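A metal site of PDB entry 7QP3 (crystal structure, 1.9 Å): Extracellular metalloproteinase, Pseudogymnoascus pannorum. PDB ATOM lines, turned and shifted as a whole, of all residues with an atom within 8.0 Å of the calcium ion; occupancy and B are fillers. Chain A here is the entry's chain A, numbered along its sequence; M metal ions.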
ATOM      1  N   GLN A  53       3.073  -1.274  -0.153  1.00  0.00           N
ATOM      2  CA  GLN A  53       3.866  -0.087  -0.420  1.00  0.00           C
ATOM      3  C   GLN A  53       3.565   0.411  -1.822  1.00  0.00           C
ATOM      4  O   GLN A  53       3.017  -0.309  -2.653  1.00  0.00           O
ATOM      5  CB  GLN A  53       5.378  -0.359  -0.284  1.00  0.00           C
ATOM      6  CG  GLN A  53       5.878  -1.549  -1.073  1.00  0.00           C
ATOM      7  CD  GLN A  53       5.484  -2.857  -0.414  1.00  0.00           C
ATOM      8  OE1 GLN A  53       5.563  -2.995   0.804  1.00  0.00           O
ATOM      9  NE2 GLN A  53       5.029  -3.801  -1.205  1.00  0.00           N
ATOM     10  N   ALA A  54       3.969   1.654  -2.077  1.00  0.00           N
ATOM     11  CA  ALA A  54       3.898   2.266  -3.399  1.00  0.00           C
ATOM     12  C   ALA A  54       5.119   1.819  -4.177  1.00  0.00           C
ATOM     13  O   ALA A  54       6.199   2.397  -4.046  1.00  0.00           O
ATOM     14  CB  ALA A  54       3.845   3.785  -3.281  1.00  0.00           C
ATOM     15  N   ASN A  55       4.964   0.789  -4.983  1.00  0.00           N
ATOM     16  CA  ASN A  55       6.070   0.262  -5.769  1.00  0.00           C
ATOM     17  C   ASN A  55       6.155   0.993  -7.124  1.00  0.00           C
ATOM     18  O   ASN A  55       6.072   0.407  -8.208  1.00  0.00           O
ATOM     19  CB  ASN A  55       5.899  -1.247  -5.947  1.00  0.00           C
ATOM     20  CG  ASN A  55       7.183  -1.966  -6.241  1.00  0.00           C
ATOM     21  OD1 ASN A  55       8.197  -1.797  -5.552  1.00  0.00           O
ATOM     22  ND2 ASN A  55       7.142  -2.818  -7.272  1.00  0.00           N
ATOM     23  N   TYR A  56       6.354   2.315  -7.036  1.00  0.00           N
ATOM     24  CA  TYR A  56       6.509   3.134  -8.241  1.00  0.00           C
ATOM     25  C   TYR A  56       7.644   2.661  -9.140  1.00  0.00           C
ATOM     26  O   TYR A  56       7.591   2.867 -10.362  1.00  0.00           O
ATOM     27  CB  TYR A  56       6.807   4.575  -7.893  1.00  0.00           C
ATOM     28  CG  TYR A  56       5.779   5.330  -7.091  1.00  0.00           C
ATOM     29  CD1 TYR A  56       4.412   5.120  -7.240  1.00  0.00           C
ATOM     30  CD2 TYR A  56       6.209   6.305  -6.192  1.00  0.00           C
ATOM     31  CE1 TYR A  56       3.496   5.853  -6.487  1.00  0.00           C
ATOM     32  CE2 TYR A  56       5.324   7.031  -5.463  1.00  0.00           C
ATOM     33  CZ  TYR A  56       3.977   6.812  -5.600  1.00  0.00           C
ATOM     34  OH  TYR A  56       3.121   7.566  -4.842  1.00  0.00           O
ATOM     35  N   ASP A  57       8.701   2.083  -8.568  1.00  0.00           N
ATOM     36  CA  ASP A  57       9.846   1.630  -9.359  1.00  0.00           C
ATOM     37  C   ASP A  57       9.525   0.385 -10.167  1.00  0.00           C
ATOM     38  O   ASP A  57      10.306   0.034 -11.063  1.00  0.00           O
ATOM     39  CB  ASP A  57      11.086   1.375  -8.478  1.00  0.00           C
ATOM     40  CG  ASP A  57      10.838   0.351  -7.348  1.00  0.00           C
ATOM     41  OD1 ASP A  57       9.870  -0.435  -7.401  1.00  0.00           O
ATOM     42  OD2 ASP A  57      11.631   0.356  -6.379  1.00  0.00           O
ATOM     43  N   GLY A  58       8.408  -0.273  -9.884  1.00  0.00           N
ATOM     44  CA  GLY A  58       8.022  -1.479 -10.571  1.00  0.00           C
ATOM     45  C   GLY A  58       8.949  -2.661 -10.368  1.00  0.00           C
ATOM     46  O   GLY A  58       8.832  -3.649 -11.088  1.00  0.00           O
ATOM     47  N   ASP A  59       9.854  -2.591  -9.389  1.00  0.00           N
ATOM     48  CA  ASP A  59      10.879  -3.618  -9.273  1.00  0.00           C
ATOM     49  C   ASP A  59      10.447  -4.715  -8.295  1.00  0.00           C
ATOM     50  O   ASP A  59       9.277  -4.812  -7.902  1.00  0.00           O
ATOM     51  CB  ASP A  59      12.228  -2.968  -8.914  1.00  0.00           C
ATOM     52  CG  ASP A  59      12.365  -2.521  -7.448  1.00  0.00           C
ATOM     53  OD1 ASP A  59      11.461  -2.699  -6.599  1.00  0.00           O
ATOM     54  OD2 ASP A  59      13.446  -1.975  -7.122  1.00  0.00           O
ATOM     55  N   ASN A  60      11.377  -5.609  -7.975  1.00  0.00           N
ATOM     56  CA  ASN A  60      11.127  -6.780  -7.153  1.00  0.00           C
ATOM     57  C   ASN A  60      11.426  -6.551  -5.693  1.00  0.00           C
ATOM     58  O   ASN A  60      11.335  -7.498  -4.917  1.00  0.00           O
ATOM     59  CB  ASN A  60      12.002  -7.954  -7.624  1.00  0.00           C
ATOM     60  CG  ASN A  60      11.595  -8.465  -8.987  1.00  0.00           C
ATOM     61  OD1 ASN A  60      10.451  -8.301  -9.396  1.00  0.00           O
ATOM     62  ND2 ASN A  60      12.533  -9.088  -9.696  1.00  0.00           N
ATOM     63  N   SER A  61      11.804  -5.338  -5.303  1.00  0.00           N
ATOM     64  CA  SER A  61      12.106  -5.018  -3.918  1.00  0.00           C
ATOM     65  C   SER A  61      10.965  -4.235  -3.306  1.00  0.00           C
ATOM     66  O   SER A  61      10.391  -3.351  -3.944  1.00  0.00           O
ATOM     67  CB  SER A  61      13.401  -4.201  -3.832  1.00  0.00           C
ATOM     68  OG  SER A  61      13.634  -3.798  -2.494  1.00  0.00           O
ATOM     69  N   TRP A  62      10.628  -4.549  -2.059  1.00  0.00           N
ATOM     70  CA  TRP A  62       9.654  -3.774  -1.327  1.00  0.00           C
ATOM     71  C   TRP A  62      10.266  -3.000  -0.162  1.00  0.00           C
ATOM     72  O   TRP A  62       9.531  -2.455   0.669  1.00  0.00           O
ATOM     73  CB  TRP A  62       8.570  -4.688  -0.805  1.00  0.00           C
ATOM     74  CG  TRP A  62       9.082  -5.714   0.115  1.00  0.00           C
ATOM     75  CD1 TRP A  62       9.262  -5.611   1.473  1.00  0.00           C
ATOM     76  CD2 TRP A  62       9.465  -7.042  -0.233  1.00  0.00           C
ATOM     77  NE1 TRP A  62       9.732  -6.784   1.982  1.00  0.00           N
ATOM     78  CE2 TRP A  62       9.879  -7.682   0.959  1.00  0.00           C
ATOM     79  CE3 TRP A  62       9.523  -7.741  -1.433  1.00  0.00           C
ATOM     80  CZ2 TRP A  62      10.331  -9.003   0.968  1.00  0.00           C
ATOM     81  CZ3 TRP A  62       9.980  -9.054  -1.419  1.00  0.00           C
ATOM     82  CH2 TRP A  62      10.372  -9.678  -0.228  1.00  0.00           C
ATOM     83  N   THR A  63      11.596  -2.944  -0.079  1.00  0.00           N
ATOM     84  CA  THR A  63      12.304  -2.190   0.967  1.00  0.00           C
ATOM     85  C   THR A  63      12.870  -0.870   0.480  1.00  0.00           C
ATOM     86  O   THR A  63      13.554  -0.198   1.252  1.00  0.00           O
ATOM     87  CB  THR A  63      13.464  -3.005   1.546  1.00  0.00           C
ATOM     88  OG1 THR A  63      14.420  -3.311   0.513  1.00  0.00           O
ATOM     89  CG2 THR A  63      12.937  -4.312   2.181  1.00  0.00           C
ATOM     90  N   ASN A  64      12.628  -0.507  -0.787  1.00  0.00           N
ATOM     91  CA  ASN A  64      13.104   0.753  -1.338  1.00  0.00           C
ATOM     92  C   ASN A  64      11.924   1.619  -1.759  1.00  0.00           C
ATOM     93  O   ASN A  64      12.043   2.468  -2.653  1.00  0.00           O
ATOM     94  CB  ASN A  64      14.066   0.513  -2.519  1.00  0.00           C
ATOM     95  CG  ASN A  64      13.433  -0.277  -3.658  1.00  0.00           C
ATOM     96  OD1 ASN A  64      12.263  -0.658  -3.580  1.00  0.00           O
ATOM     97  ND2 ASN A  64      14.200  -0.518  -4.724  1.00  0.00           N
ATOM     98  N   ASP A  65      10.788   1.443  -1.097  1.00  0.00           N
ATOM     99  CA  ASP A  65       9.558   2.097  -1.484  1.00  0.00           C
ATOM    100  C   ASP A  65       8.955   2.866  -0.332  1.00  0.00           C
ATOM    101  O   ASP A  65       9.075   2.478   0.833  1.00  0.00           O
ATOM    102  CB  ASP A  65       8.533   1.085  -1.961  1.00  0.00           C
ATOM    103  CG  ASP A  65       9.062   0.225  -3.065  1.00  0.00           C
ATOM    104  OD1 ASP A  65       9.390   0.779  -4.130  1.00  0.00           O
ATOM    105  OD2 ASP A  65       9.187  -0.997  -2.860  1.00  0.00           O
ATOM    106  N   TYR A  66       8.241   3.920  -0.687  1.00  0.00           N
ATOM    107  CA  TYR A  66       7.436   4.639   0.301  1.00  0.00           C
ATOM    108  C   TYR A  66       6.289   3.756   0.764  1.00  0.00           C
ATOM    109  O   TYR A  66       5.633   3.083  -0.039  1.00  0.00           O
ATOM    110  CB  TYR A  66       6.881   5.929  -0.287  1.00  0.00           C
ATOM    111  CG  TYR A  66       5.856   6.577   0.585  1.00  0.00           C
ATOM    112  CD1 TYR A  66       6.230   7.319   1.684  1.00  0.00           C
ATOM    113  CD2 TYR A  66       4.513   6.413   0.319  1.00  0.00           C
ATOM    114  CE1 TYR A  66       5.277   7.895   2.521  1.00  0.00           C
ATOM    115  CE2 TYR A  66       3.539   6.996   1.127  1.00  0.00           C
ATOM    116  CZ  TYR A  66       3.935   7.720   2.227  1.00  0.00           C
ATOM    117  OH  TYR A  66       3.006   8.291   3.046  1.00  0.00           O
ATOM    118  N   ILE A 136       3.240  -9.570  -1.000  1.00  0.00           N
ATOM    119  CA  ILE A 136       3.815  -8.273  -1.316  1.00  0.00           C
ATOM    120  C   ILE A 136       2.764  -7.516  -2.120  1.00  0.00           C
ATOM    121  O   ILE A 136       2.342  -7.973  -3.187  1.00  0.00           O
ATOM    122  CB  ILE A 136       5.122  -8.403  -2.113  1.00  0.00           C
ATOM    123  CG1 ILE A 136       6.080  -9.378  -1.430  1.00  0.00           C
ATOM    124  CG2 ILE A 136       5.793  -7.034  -2.326  1.00  0.00           C
ATOM    125  CD1 ILE A 136       6.281  -9.089   0.051  1.00  0.00           C
ATOM    126  N   ASN A 138       1.810  -4.374  -4.036  1.00  0.00           N
ATOM    127  CA  ASN A 138       2.422  -3.236  -4.725  1.00  0.00           C
ATOM    128  C   ASN A 138       1.336  -2.338  -5.299  1.00  0.00           C
ATOM    129  O   ASN A 138       0.730  -2.649  -6.316  1.00  0.00           O
ATOM    130  CB  ASN A 138       3.363  -3.738  -5.786  1.00  0.00           C
ATOM    131  CG  ASN A 138       4.537  -4.451  -5.185  1.00  0.00           C
ATOM    132  OD1 ASN A 138       5.126  -3.994  -4.219  1.00  0.00           O
ATOM    133  ND2 ASN A 138       4.856  -5.572  -5.729  1.00  0.00           N
ATOM    134  N   ASP A 141       1.905   0.258  -9.008  1.00  0.00           N
ATOM    135  CA  ASP A 141       3.138  -0.373  -9.462  1.00  0.00           C
ATOM    136  C   ASP A 141       3.523   0.179 -10.821  1.00  0.00           C
ATOM    137  O   ASP A 141       2.691   0.288 -11.726  1.00  0.00           O
ATOM    138  CB  ASP A 141       2.942  -1.884  -9.504  1.00  0.00           C
ATOM    139  CG  ASP A 141       4.230  -2.630  -9.784  1.00  0.00           C
ATOM    140  OD1 ASP A 141       4.713  -2.539 -10.923  1.00  0.00           O
ATOM    141  OD2 ASP A 141       4.768  -3.279  -8.864  1.00  0.00           O
ATOM    142  N   ARG A 162       0.609  -6.929  -8.039  1.00  0.00           N
ATOM    143  CA  ARG A 162       0.932  -5.639  -8.634  1.00  0.00           C
ATOM    144  C   ARG A 162      -0.358  -5.022  -9.153  1.00  0.00           C
ATOM    145  O   ARG A 162      -1.076  -5.647  -9.935  1.00  0.00           O
ATOM    146  CB  ARG A 162       1.961  -5.766  -9.761  1.00  0.00           C
ATOM    147  CG  ARG A 162       3.279  -6.337  -9.300  1.00  0.00           C
ATOM    148  CD  ARG A 162       4.258  -6.438 -10.452  1.00  0.00           C
ATOM    149  NE  ARG A 162       5.457  -7.190 -10.075  1.00  0.00           N
ATOM    150  CZ  ARG A 162       6.568  -6.645  -9.610  1.00  0.00           C
ATOM    151  NH1 ARG A 162       6.689  -5.337  -9.435  1.00  0.00           N
ATOM    152  NH2 ARG A 162       7.582  -7.441  -9.277  1.00  0.00           N
HETATM  153 CA    CA M   1      10.372  -1.228  -5.042  1.00  0.00          CA
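The side-chain hydroxyl (OG) of Ser 61 lies within hydrogen-bond range of the side-chain hydroxyl (OG1) of Thr 63.
The side-chain amide nitrogen (ND2) of Asn 55 sits close to the guanidinium group (NH1) of Arg 162 (3.4 Å).
The guanidinium group of Arg 162 is in hydrogen-bond range of the backbone carbonyl oxygen of Asp 59.
The side-chain amide nitrogen (ND2) of Asn 55 is in hydrogen-bond range of the side-chain carboxylate (OD2) of Asp 141.
The nearest printed residue that does not touch the calcium ion is Trp 62 (4.5 Å).
The calcium ion is bound by OD1 of Asn 55, O of Ser 61, OD1 of Asp 59, OD1 of Asp 65, OD2 of Asp 57, OD1 of Asn 64, OD2 of Asp 65 and OD1 of Asp 57.
The calcium ion has eight donor atoms within binding distance.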
